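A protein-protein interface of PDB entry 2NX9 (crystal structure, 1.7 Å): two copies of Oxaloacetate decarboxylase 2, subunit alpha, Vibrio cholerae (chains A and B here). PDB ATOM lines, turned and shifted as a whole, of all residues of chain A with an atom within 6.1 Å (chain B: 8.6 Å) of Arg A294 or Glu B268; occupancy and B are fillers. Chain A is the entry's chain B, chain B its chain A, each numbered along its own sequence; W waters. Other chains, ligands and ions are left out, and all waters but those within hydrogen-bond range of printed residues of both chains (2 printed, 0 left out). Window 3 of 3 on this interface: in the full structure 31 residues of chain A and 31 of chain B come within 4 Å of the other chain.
The side-chain carboxylate of Glu B247 lies within hydrogen-bond range of the side-chain hydroxyl of Ser B235 (2.6 Å).
The side-chain carboxylate (OD1) of Asp A292 lies within salt-bridge range of the guanidinium group (NE) of Arg A294, at 3.0 Å.
Among the printed residues, pairs that only touch across the chains: Met A288 with Arg B275, Ala A293 with Ser B235, Ala A293 with Glu B247, Ala A293 with Glu B268, Arg A294 with Glu B268, Leu A296 with Glu B247 and Leu A296 with Ile B264.
Arg A294 touches just one residue of chain B: Glu B268.
Glu B268 touches just these residues of chain A: Ala A293 (3.9 Å) and Arg A294 (3.0 Å).
Ala A293 touches just these residues of chain B: Ser B235, Glu B247 and Glu B268.
Of the printed residues of chain A, Ile B264 touches Leu A296.
Of the printed residues of chain B, Met A288 touches Arg B275.
Of the printed residues of chain A, Glu B247 touches Ala A293 and Leu A296.
Of the printed residues of chain A, Arg B275 touches Met A288 (3.4 Å).
Of the printed residues of chain B, Leu A296 touches Glu B247 (3.4 Å) and Ile B264 (3.7 Å).
Ala B272 touches none of the printed residues of chain A.
Thr B246 touches none of the printed residues of chain A.
The nearest residue of chain A that does not touch Glu B268 is Val A297 (4.1 Å).
The nearest printed residue of chain B that does not touch Met A288 is Ser B235 (6.9 Å).
Of the 14 printed residues of chain A, 4 touch a printed residue of chain B.
Printed residues of chain A that touch a printed residue of chain B: Met A288, Ala A293, Arg A294 and Leu A296.
Hydrophobic or aromatic side chains of chain B that line the printed part of chain A: Ile B264.
No position is printed for both chains.
Of the 7 pairs that touch across the chains among the printed residues, none has its exchanged pair printed and touching as well.
Water W2 lies within hydrogen-bond range of OG of Ser B235 (2.7 Å), N of Ala A293 (3.0 Å) and NH2 of Arg B275 (3.5 Å).
Water W1 lies within hydrogen-bond range of the guanidinium group of Arg B275 (2.9 Å), the side-chain carboxylate of Asp A292 (3.4 Å) and the guanidinium group of Arg A294 (3.4 Å).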
ATOM      1  N   MET A 288       3.915  12.537  23.489  1.00  0.00           N
ATOM      2  CA  MET A 288       3.111  13.476  24.237  1.00  0.00           C
ATOM      3  C   MET A 288       3.081  13.080  25.705  1.00  0.00           C
ATOM      4  O   MET A 288       2.911  11.900  26.055  1.00  0.00           O
ATOM      5  CB  MET A 288       1.699  13.554  23.664  1.00  0.00           C
ATOM      6  CG  MET A 288       0.923  14.820  24.031  1.00  0.00           C
ATOM      7  SD  MET A 288      -0.557  14.507  24.995  1.00  0.00           S
ATOM      8  CE  MET A 288      -1.370  13.263  24.031  1.00  0.00           C
ATOM      9  N   ASP A 292      -2.969  17.469  25.331  1.00  0.00           N
ATOM     10  CA  ASP A 292      -2.656  18.317  24.175  1.00  0.00           C
ATOM     11  C   ASP A 292      -3.655  19.469  24.076  1.00  0.00           C
ATOM     12  O   ASP A 292      -4.790  19.291  23.614  1.00  0.00           O
ATOM     13  CB  ASP A 292      -2.667  17.452  22.896  1.00  0.00           C
ATOM     14  CG  ASP A 292      -1.922  18.093  21.730  1.00  0.00           C
ATOM     15  OD1 ASP A 292      -1.647  19.309  21.759  1.00  0.00           O
ATOM     16  OD2 ASP A 292      -1.599  17.357  20.770  1.00  0.00           O
ATOM     17  N   ALA A 293      -3.226  20.646  24.526  1.00  0.00           N
ATOM     18  CA  ALA A 293      -4.087  21.830  24.596  1.00  0.00           C
ATOM     19  C   ALA A 293      -4.217  22.535  23.267  1.00  0.00           C
ATOM     20  O   ALA A 293      -5.044  23.435  23.142  1.00  0.00           O
ATOM     21  CB  ALA A 293      -3.566  22.811  25.615  1.00  0.00           C
ATOM     22  N   ARG A 294      -3.418  22.127  22.285  1.00  0.00           N
ATOM     23  CA  ARG A 294      -3.551  22.648  20.932  1.00  0.00           C
ATOM     24  C   ARG A 294      -4.880  22.188  20.329  1.00  0.00           C
ATOM     25  O   ARG A 294      -5.513  22.908  19.570  1.00  0.00           O
ATOM     26  CB  ARG A 294      -2.368  22.241  20.045  1.00  0.00           C
ATOM     27  CG  ARG A 294      -1.001  22.657  20.546  1.00  0.00           C
ATOM     28  CD  ARG A 294       0.120  22.085  19.698  1.00  0.00           C
ATOM     29  NE  ARG A 294       0.163  20.629  19.831  1.00  0.00           N
ATOM     30  CZ  ARG A 294       1.102  19.844  19.319  1.00  0.00           C
ATOM     31  NH1 ARG A 294       2.117  20.360  18.633  1.00  0.00           N
ATOM     32  NH2 ARG A 294       1.031  18.533  19.506  1.00  0.00           N
ATOM     33  N   ILE A 295      -5.315  20.985  20.646  1.00  0.00           N
ATOM     34  CA  ILE A 295      -6.619  20.539  20.183  1.00  0.00           C
ATOM     35  C   ILE A 295      -7.752  21.495  20.657  1.00  0.00           C
ATOM     36  O   ILE A 295      -8.722  21.718  19.935  1.00  0.00           O
ATOM     37  CB  ILE A 295      -6.875  19.060  20.575  1.00  0.00           C
ATOM     38  CG1 ILE A 295      -5.777  18.144  19.994  1.00  0.00           C
ATOM     39  CG2 ILE A 295      -8.265  18.615  20.115  1.00  0.00           C
ATOM     40  CD1 ILE A 295      -5.595  16.770  20.743  1.00  0.00           C
ATOM     41  N   LEU A 296      -7.577  22.115  21.826  1.00  0.00           N
ATOM     42  CA  LEU A 296      -8.621  22.919  22.462  1.00  0.00           C
ATOM     43  C   LEU A 296      -8.769  24.310  21.856  1.00  0.00           C
ATOM     44  O   LEU A 296      -9.793  24.968  22.049  1.00  0.00           O
ATOM     45  CB  LEU A 296      -8.377  23.052  23.977  1.00  0.00           C
ATOM     46  CG  LEU A 296      -8.422  21.780  24.851  1.00  0.00           C
ATOM     47  CD1 LEU A 296      -8.157  22.121  26.286  1.00  0.00           C
ATOM     48  CD2 LEU A 296      -9.759  21.094  24.742  1.00  0.00           C
ATOM     49  N   VAL A 297      -7.754  24.753  21.130  1.00  0.00           N
ATOM     50  CA  VAL A 297      -7.744  26.110  20.572  1.00  0.00           C
ATOM     51  C   VAL A 297      -8.820  26.293  19.514  1.00  0.00           C
ATOM     52  O   VAL A 297      -9.508  27.325  19.504  1.00  0.00           O
ATOM     53  CB  VAL A 297      -6.369  26.510  20.018  1.00  0.00           C
ATOM     54  CG1 VAL A 297      -6.440  27.873  19.341  1.00  0.00           C
ATOM     55  CG2 VAL A 297      -5.361  26.557  21.143  1.00  0.00           C
ATOM     56  N   ALA A 298      -8.975  25.297  18.639  1.00  0.00           N
ATOM     57  CA  ALA A 298      -9.889  25.397  17.496  1.00  0.00           C
ATOM     58  C   ALA A 298     -10.368  24.080  16.891  1.00  0.00           C
ATOM     59  O   ALA A 298     -10.877  24.058  15.774  1.00  0.00           O
ATOM     60  CB  ALA A 298      -9.337  26.374  16.427  1.00  0.00           C
ATOM     61  N   GLN A 299     -10.182  22.997  17.638  1.00  0.00           N
ATOM     62  CA  GLN A 299     -10.779  21.681  17.343  1.00  0.00           C
ATOM     63  C   GLN A 299     -10.065  20.939  16.208  1.00  0.00           C
ATOM     64  O   GLN A 299     -10.666  20.098  15.531  1.00  0.00           O
ATOM     65  CB  GLN A 299     -12.306  21.727  17.114  1.00  0.00           C
ATOM     66  CG  GLN A 299     -13.138  21.782  18.395  1.00  0.00           C
ATOM     67  CD  GLN A 299     -13.023  23.113  19.107  1.00  0.00           C
ATOM     68  OE1 GLN A 299     -12.581  23.179  20.253  1.00  0.00           O
ATOM     69  NE2 GLN A 299     -13.405  24.189  18.425  1.00  0.00           N
ATOM     70  N   VAL A 300      -8.791  21.241  15.995  1.00  0.00           N
ATOM     71  CA  VAL A 300      -8.005  20.498  15.020  1.00  0.00           C
ATOM     72  C   VAL A 300      -7.519  19.245  15.733  1.00  0.00           C
ATOM     73  O   VAL A 300      -6.816  19.356  16.737  1.00  0.00           O
ATOM     74  CB  VAL A 300      -6.778  21.301  14.517  1.00  0.00           C
ATOM     75  CG1 VAL A 300      -6.009  20.500  13.475  1.00  0.00           C
ATOM     76  CG2 VAL A 300      -7.190  22.670  13.944  1.00  0.00           C
ATOM     77  N   GLY A 302      -5.315  16.063  16.879  1.00  0.00           N
ATOM     78  CA  GLY A 302      -3.863  15.923  17.023  1.00  0.00           C
ATOM     79  C   GLY A 302      -3.196  15.266  15.831  1.00  0.00           C
ATOM     80  O   GLY A 302      -2.158  15.738  15.360  1.00  0.00           O
ATOM     81  N   LEU A 305      -3.025  17.741  12.822  1.00  0.00           N
ATOM     82  CA  LEU A 305      -1.910  18.692  12.990  1.00  0.00           C
ATOM     83  C   LEU A 305      -0.569  18.023  12.711  1.00  0.00           C
ATOM     84  O   LEU A 305       0.189  18.478  11.870  1.00  0.00           O
ATOM     85  CB  LEU A 305      -1.894  19.326  14.389  1.00  0.00           C
ATOM     86  CG  LEU A 305      -0.757  20.321  14.702  1.00  0.00           C
ATOM     87  CD1 LEU A 305      -0.804  21.554  13.808  1.00  0.00           C
ATOM     88  CD2 LEU A 305      -0.755  20.744  16.162  1.00  0.00           C
ATOM     89  N   THR A 306      -0.292  16.937  13.427  1.00  0.00           N
ATOM     90  CA  THR A 306       0.917  16.151  13.203  1.00  0.00           C
ATOM     91  C   THR A 306       1.170  15.953  11.710  1.00  0.00           C
ATOM     92  O   THR A 306       2.276  16.196  11.225  1.00  0.00           O
ATOM     93  CB  THR A 306       0.833  14.795  13.929  1.00  0.00           C
ATOM     94  OG1 THR A 306       0.586  15.027  15.317  1.00  0.00           O
ATOM     95  CG2 THR A 306       2.122  14.015  13.781  1.00  0.00           C
ATOM     96  N   GLU A 309       1.943  19.279   9.781  1.00  0.00           N
ATOM     97  CA  GLU A 309       3.287  19.771  10.066  1.00  0.00           C
ATOM     98  C   GLU A 309       4.378  18.949   9.373  1.00  0.00           C
ATOM     99  O   GLU A 309       5.388  19.513   8.951  1.00  0.00           O
ATOM    100  CB  GLU A 309       3.534  19.940  11.571  1.00  0.00           C
ATOM    101  CG  GLU A 309       3.462  18.671  12.385  1.00  0.00           C
ATOM    102  CD  GLU A 309       3.547  18.931  13.884  1.00  0.00           C
ATOM    103  OE1 GLU A 309       3.199  20.061  14.318  1.00  0.00           O
ATOM    104  OE2 GLU A 309       3.967  18.001  14.622  1.00  0.00           O
ATOM    105  N   ILE B  35       9.477  32.245  30.675  1.00  0.00           N
ATOM    106  CA  ILE B  35       8.007  32.144  30.521  1.00  0.00           C
ATOM    107  C   ILE B  35       7.213  32.837  31.630  1.00  0.00           C
ATOM    108  O   ILE B  35       5.998  32.724  31.665  1.00  0.00           O
ATOM    109  CB  ILE B  35       7.530  30.687  30.435  1.00  0.00           C
ATOM    110  CG1 ILE B  35       6.145  30.604  29.799  1.00  0.00           C
ATOM    111  CG2 ILE B  35       7.509  30.074  31.797  1.00  0.00           C
ATOM    112  CD1 ILE B  35       6.139  30.881  28.313  1.00  0.00           C
ATOM    113  N   GLN B  38       4.532  35.576  30.855  1.00  0.00           N
ATOM    114  CA  GLN B  38       3.335  35.098  30.203  1.00  0.00           C
ATOM    115  C   GLN B  38       2.400  34.454  31.225  1.00  0.00           C
ATOM    116  O   GLN B  38       1.187  34.680  31.179  1.00  0.00           O
ATOM    117  CB  GLN B  38       3.659  34.171  29.035  1.00  0.00           C
ATOM    118  CG  GLN B  38       3.975  34.926  27.751  1.00  0.00           C
ATOM    119  CD  GLN B  38       4.216  34.023  26.546  1.00  0.00           C
ATOM    120  OE1 GLN B  38       3.450  33.090  26.273  1.00  0.00           O
ATOM    121  NE2 GLN B  38       5.280  34.318  25.802  1.00  0.00           N
ATOM    122  N   ILE B  42      -1.899  35.828  32.703  1.00  0.00           N
ATOM    123  CA  ILE B  42      -3.024  34.888  32.529  1.00  0.00           C
ATOM    124  C   ILE B  42      -4.268  35.269  33.339  1.00  0.00           C
ATOM    125  O   ILE B  42      -5.380  35.223  32.807  1.00  0.00           O
ATOM    126  CB  ILE B  42      -2.640  33.412  32.842  1.00  0.00           C
ATOM    127  CG1 ILE B  42      -1.626  32.889  31.820  1.00  0.00           C
ATOM    128  CG2 ILE B  42      -3.877  32.503  32.813  1.00  0.00           C
ATOM    129  CD1 ILE B  42      -2.166  32.783  30.377  1.00  0.00           C
ATOM    130  N   TYR B  44      -4.480  34.035  36.781  1.00  0.00           N
ATOM    131  CA  TYR B  44      -4.541  32.981  37.799  1.00  0.00           C
ATOM    132  C   TYR B  44      -4.782  33.597  39.146  1.00  0.00           C
ATOM    133  O   TYR B  44      -4.304  34.679  39.406  1.00  0.00           O
ATOM    134  CB  TYR B  44      -3.192  32.316  37.923  1.00  0.00           C
ATOM    135  CG  TYR B  44      -2.847  31.401  36.800  1.00  0.00           C
ATOM    136  CD1 TYR B  44      -3.662  30.330  36.474  1.00  0.00           C
ATOM    137  CD2 TYR B  44      -1.669  31.600  36.079  1.00  0.00           C
ATOM    138  CE1 TYR B  44      -3.331  29.545  35.455  1.00  0.00           C
ATOM    139  CE2 TYR B  44      -1.302  30.768  35.067  1.00  0.00           C
ATOM    140  CZ  TYR B  44      -2.135  29.720  34.772  1.00  0.00           C
ATOM    141  OH  TYR B  44      -1.799  28.857  33.745  1.00  0.00           O
ATOM    142  N   ILE B 234      -0.398  23.380  34.001  1.00  0.00           N
ATOM    143  CA  ILE B 234      -0.347  23.675  32.550  1.00  0.00           C
ATOM    144  C   ILE B 234      -0.375  22.349  31.858  1.00  0.00           C
ATOM    145  O   ILE B 234       0.272  21.459  32.356  1.00  0.00           O
ATOM    146  CB  ILE B 234       0.959  24.449  32.196  1.00  0.00           C
ATOM    147  CG1 ILE B 234       0.821  25.911  32.627  1.00  0.00           C
ATOM    148  CG2 ILE B 234       1.328  24.391  30.698  1.00  0.00           C
ATOM    149  CD1 ILE B 234      -0.110  26.756  31.752  1.00  0.00           C
ATOM    150  N   SER B 235      -1.122  22.212  30.756  1.00  0.00           N
ATOM    151  CA  SER B 235      -1.338  20.896  30.106  1.00  0.00           C
ATOM    152  C   SER B 235      -0.103  20.017  29.965  1.00  0.00           C
ATOM    153  O   SER B 235      -0.123  18.869  30.378  1.00  0.00           O
ATOM    154  CB  SER B 235      -1.988  21.038  28.735  1.00  0.00           C
ATOM    155  OG  SER B 235      -1.263  21.955  27.923  1.00  0.00           O
ATOM    156  N   SER B 236       0.971  20.563  29.390  1.00  0.00           N
ATOM    157  CA  SER B 236       2.185  19.756  29.084  1.00  0.00           C
ATOM    158  C   SER B 236       2.927  19.291  30.334  1.00  0.00           C
ATOM    159  O   SER B 236       3.717  18.313  30.301  1.00  0.00           O
ATOM    160  CB  SER B 236       3.109  20.498  28.120  1.00  0.00           C
ATOM    161  OG  SER B 236       3.265  21.820  28.565  1.00  0.00           O
ATOM    162  N   THR B 246      -4.809  22.557  33.267  1.00  0.00           N
ATOM    163  CA  THR B 246      -5.477  23.851  33.286  1.00  0.00           C
ATOM    164  C   THR B 246      -6.409  24.138  32.116  1.00  0.00           C
ATOM    165  O   THR B 246      -7.588  24.476  32.322  1.00  0.00           O
ATOM    166  CB  THR B 246      -4.435  24.935  33.368  1.00  0.00           C
ATOM    167  OG1 THR B 246      -3.599  24.651  34.493  1.00  0.00           O
ATOM    168  CG2 THR B 246      -5.094  26.302  33.463  1.00  0.00           C
ATOM    169  N   GLU B 247      -5.885  24.014  30.899  1.00  0.00           N
ATOM    170  CA  GLU B 247      -6.651  24.254  29.680  1.00  0.00           C
ATOM    171  C   GLU B 247      -7.917  23.399  29.597  1.00  0.00           C
ATOM    172  O   GLU B 247      -8.962  23.866  29.148  1.00  0.00           O
ATOM    173  CB  GLU B 247      -5.781  23.991  28.449  1.00  0.00           C
ATOM    174  CG  GLU B 247      -4.606  24.943  28.295  1.00  0.00           C
ATOM    175  CD  GLU B 247      -3.305  24.432  28.931  1.00  0.00           C
ATOM    176  OE1 GLU B 247      -3.302  24.121  30.138  1.00  0.00           O
ATOM    177  OE2 GLU B 247      -2.274  24.356  28.214  1.00  0.00           O
ATOM    178  N   ASP B 263      -7.654  32.205  28.993  1.00  0.00           N
ATOM    179  CA  ASP B 263      -7.609  32.147  27.534  1.00  0.00           C
ATOM    180  C   ASP B 263      -6.830  30.944  27.072  1.00  0.00           C
ATOM    181  O   ASP B 263      -5.611  30.895  27.217  1.00  0.00           O
ATOM    182  CB  ASP B 263      -7.007  33.436  26.955  1.00  0.00           C
ATOM    183  CG  ASP B 263      -7.011  33.465  25.423  1.00  0.00           C
ATOM    184  OD1 ASP B 263      -8.093  33.571  24.804  1.00  0.00           O
ATOM    185  OD2 ASP B 263      -5.919  33.404  24.830  1.00  0.00           O
ATOM    186  N   ILE B 264      -7.546  29.979  26.509  1.00  0.00           N
ATOM    187  CA  ILE B 264      -6.951  28.744  26.029  1.00  0.00           C
ATOM    188  C   ILE B 264      -5.728  28.979  25.139  1.00  0.00           C
ATOM    189  O   ILE B 264      -4.723  28.281  25.300  1.00  0.00           O
ATOM    190  CB  ILE B 264      -7.978  27.817  25.324  1.00  0.00           C
ATOM    191  CG1 ILE B 264      -9.130  27.457  26.276  1.00  0.00           C
ATOM    192  CG2 ILE B 264      -7.310  26.521  24.878  1.00  0.00           C
ATOM    193  CD1 ILE B 264     -10.264  26.677  25.609  1.00  0.00           C
ATOM    194  N   ALA B 265      -5.827  29.950  24.220  1.00  0.00           N
ATOM    195  CA  ALA B 265      -4.731  30.323  23.308  1.00  0.00           C
ATOM    196  C   ALA B 265      -3.498  30.877  24.034  1.00  0.00           C
ATOM    197  O   ALA B 265      -2.376  30.457  23.744  1.00  0.00           O
ATOM    198  CB  ALA B 265      -5.220  31.311  22.235  1.00  0.00           C
ATOM    199  N   LYS B 266      -3.704  31.807  24.972  1.00  0.00           N
ATOM    200  CA  LYS B 266      -2.605  32.342  25.772  1.00  0.00           C
ATOM    201  C   LYS B 266      -2.028  31.272  26.670  1.00  0.00           C
ATOM    202  O   LYS B 266      -0.847  31.320  26.982  1.00  0.00           O
ATOM    203  CB  LYS B 266      -3.017  33.566  26.613  1.00  0.00           C
ATOM    204  CG  LYS B 266      -3.113  34.892  25.852  1.00  0.00           C
ATOM    205  CD  LYS B 266      -4.086  35.822  26.555  1.00  0.00           C
ATOM    206  CE  LYS B 266      -3.849  37.285  26.114  1.00  0.00           C
ATOM    207  NZ  LYS B 266      -3.029  37.273  24.862  1.00  0.00           N
ATOM    208  N   LEU B 267      -2.832  30.267  27.037  1.00  0.00           N
ATOM    209  CA  LEU B 267      -2.394  29.195  27.924  1.00  0.00           C
ATOM    210  C   LEU B 267      -1.618  28.139  27.171  1.00  0.00           C
ATOM    211  O   LEU B 267      -0.608  27.651  27.662  1.00  0.00           O
ATOM    212  CB  LEU B 267      -3.594  28.538  28.601  1.00  0.00           C
ATOM    213  CG  LEU B 267      -4.205  29.217  29.816  1.00  0.00           C
ATOM    214  CD1 LEU B 267      -5.592  28.655  30.135  1.00  0.00           C
ATOM    215  CD2 LEU B 267      -3.269  29.055  30.993  1.00  0.00           C
ATOM    216  N   GLU B 268      -2.098  27.812  25.969  1.00  0.00           N
ATOM    217  CA  GLU B 268      -1.455  26.870  25.071  1.00  0.00           C
ATOM    218  C   GLU B 268      -0.047  27.327  24.686  1.00  0.00           C
ATOM    219  O   GLU B 268       0.834  26.500  24.492  1.00  0.00           O
ATOM    220  CB  GLU B 268      -2.319  26.655  23.820  1.00  0.00           C
ATOM    221  CG  GLU B 268      -1.826  25.551  22.860  1.00  0.00           C
ATOM    222  CD  GLU B 268      -0.585  25.954  22.065  1.00  0.00           C
ATOM    223  OE1 GLU B 268      -0.426  27.148  21.726  1.00  0.00           O
ATOM    224  OE2 GLU B 268       0.246  25.074  21.796  1.00  0.00           O
ATOM    225  N   GLN B 269       0.174  28.632  24.553  1.00  0.00           N
ATOM    226  CA  GLN B 269       1.524  29.125  24.278  1.00  0.00           C
ATOM    227  C   GLN B 269       2.513  28.749  25.388  1.00  0.00           C
ATOM    228  O   GLN B 269       3.663  28.374  25.117  1.00  0.00           O
ATOM    229  CB  GLN B 269       1.513  30.643  24.050  1.00  0.00           C
ATOM    230  CG  GLN B 269       0.873  31.028  22.731  1.00  0.00           C
ATOM    231  CD  GLN B 269       0.937  32.523  22.448  1.00  0.00           C
ATOM    232  OE1 GLN B 269       2.013  33.131  22.474  1.00  0.00           O
ATOM    233  NE2 GLN B 269      -0.223  33.123  22.176  1.00  0.00           N
ATOM    234  N   ILE B 270       2.044  28.853  26.632  1.00  0.00           N
ATOM    235  CA  ILE B 270       2.843  28.549  27.806  1.00  0.00           C
ATOM    236  C   ILE B 270       3.057  27.040  27.855  1.00  0.00           C
ATOM    237  O   ILE B 270       4.142  26.556  28.206  1.00  0.00           O
ATOM    238  CB  ILE B 270       2.134  29.087  29.074  1.00  0.00           C
ATOM    239  CG1 ILE B 270       2.150  30.616  29.039  1.00  0.00           C
ATOM    240  CG2 ILE B 270       2.782  28.569  30.361  1.00  0.00           C
ATOM    241  CD1 ILE B 270       1.124  31.295  29.933  1.00  0.00           C
ATOM    242  N   ALA B 271       2.025  26.296  27.474  1.00  0.00           N
ATOM    243  CA  ALA B 271       2.123  24.851  27.424  1.00  0.00           C
ATOM    244  C   ALA B 271       3.181  24.414  26.409  1.00  0.00           C
ATOM    245  O   ALA B 271       3.940  23.473  26.654  1.00  0.00           O
ATOM    246  CB  ALA B 271       0.754  24.226  27.087  1.00  0.00           C
ATOM    247  N   ALA B 272       3.198  25.077  25.259  1.00  0.00           N
ATOM    248  CA  ALA B 272       4.164  24.790  24.214  1.00  0.00           C
ATOM    249  C   ALA B 272       5.570  25.017  24.751  1.00  0.00           C
ATOM    250  O   ALA B 272       6.439  24.164  24.583  1.00  0.00           O
ATOM    251  CB  ALA B 272       3.906  25.657  22.998  1.00  0.00           C
ATOM    252  N   TYR B 273       5.784  26.154  25.417  1.00  0.00           N
ATOM    253  CA  TYR B 273       7.054  26.423  26.068  1.00  0.00           C
ATOM    254  C   TYR B 273       7.470  25.291  27.003  1.00  0.00           C
ATOM    255  O   TYR B 273       8.617  24.804  26.935  1.00  0.00           O
ATOM    256  CB  TYR B 273       7.009  27.755  26.823  1.00  0.00           C
ATOM    257  CG  TYR B 273       8.243  28.038  27.659  1.00  0.00           C
ATOM    258  CD1 TYR B 273       9.338  28.717  27.125  1.00  0.00           C
ATOM    259  CD2 TYR B 273       8.319  27.603  28.979  1.00  0.00           C
ATOM    260  CE1 TYR B 273      10.473  28.965  27.899  1.00  0.00           C
ATOM    261  CE2 TYR B 273       9.430  27.826  29.747  1.00  0.00           C
ATOM    262  CZ  TYR B 273      10.507  28.514  29.213  1.00  0.00           C
ATOM    263  OH  TYR B 273      11.606  28.740  30.007  1.00  0.00           O
ATOM    264  N   PHE B 274       6.539  24.852  27.857  1.00  0.00           N
ATOM    265  CA  PHE B 274       6.858  23.836  28.855  1.00  0.00           C
ATOM    266  C   PHE B 274       7.010  22.443  28.292  1.00  0.00           C
ATOM    267  O   PHE B 274       7.610  21.596  28.938  1.00  0.00           O
ATOM    268  CB  PHE B 274       5.855  23.825  30.023  1.00  0.00           C
ATOM    269  CG  PHE B 274       6.149  24.871  31.069  1.00  0.00           C
ATOM    270  CD1 PHE B 274       7.191  24.691  31.984  1.00  0.00           C
ATOM    271  CD2 PHE B 274       5.401  26.031  31.132  1.00  0.00           C
ATOM    272  CE1 PHE B 274       7.492  25.663  32.940  1.00  0.00           C
ATOM    273  CE2 PHE B 274       5.674  26.998  32.094  1.00  0.00           C
ATOM    274  CZ  PHE B 274       6.732  26.815  32.993  1.00  0.00           C
ATOM    275  N   ARG B 275       6.459  22.200  27.105  1.00  0.00           N
ATOM    276  CA  ARG B 275       6.608  20.888  26.472  1.00  0.00           C
ATOM    277  C   ARG B 275       8.070  20.675  26.077  1.00  0.00           C
ATOM    278  O   ARG B 275       8.622  19.576  26.212  1.00  0.00           O
ATOM    279  CB  ARG B 275       5.679  20.733  25.260  1.00  0.00           C
ATOM    280  CG  ARG B 275       5.800  19.369  24.565  1.00  0.00           C
ATOM    281  CD  ARG B 275       4.645  19.085  23.601  1.00  0.00           C
ATOM    282  NE  ARG B 275       3.326  19.199  24.230  1.00  0.00           N
ATOM    283  CZ  ARG B 275       2.708  18.222  24.896  1.00  0.00           C
ATOM    284  NH1 ARG B 275       3.293  17.035  25.044  1.00  0.00           N
ATOM    285  NH2 ARG B 275       1.504  18.437  25.425  1.00  0.00           N
ATOM    286  N   ASP B 276       8.699  21.742  25.609  1.00  0.00           N
ATOM    287  CA  ASP B 276      10.096  21.680  25.221  1.00  0.00           C
ATOM    288  C   ASP B 276      10.953  21.523  26.477  1.00  0.00           C
ATOM    289  O   ASP B 276      11.820  20.650  26.516  1.00  0.00           O
ATOM    290  CB  ASP B 276      10.484  22.918  24.396  1.00  0.00           C
ATOM    291  CG  ASP B 276       9.701  23.036  23.071  1.00  0.00           C
ATOM    292  OD1 ASP B 276       9.418  21.998  22.418  1.00  0.00           O
ATOM    293  OD2 ASP B 276       9.380  24.183  22.675  1.00  0.00           O
HETATM  294  O   HOH W   1       1.169  20.730  23.114  1.00  0.00           O
HETATM  295  O   HOH W   2      -0.465  21.284  25.380  1.00  0.00           O
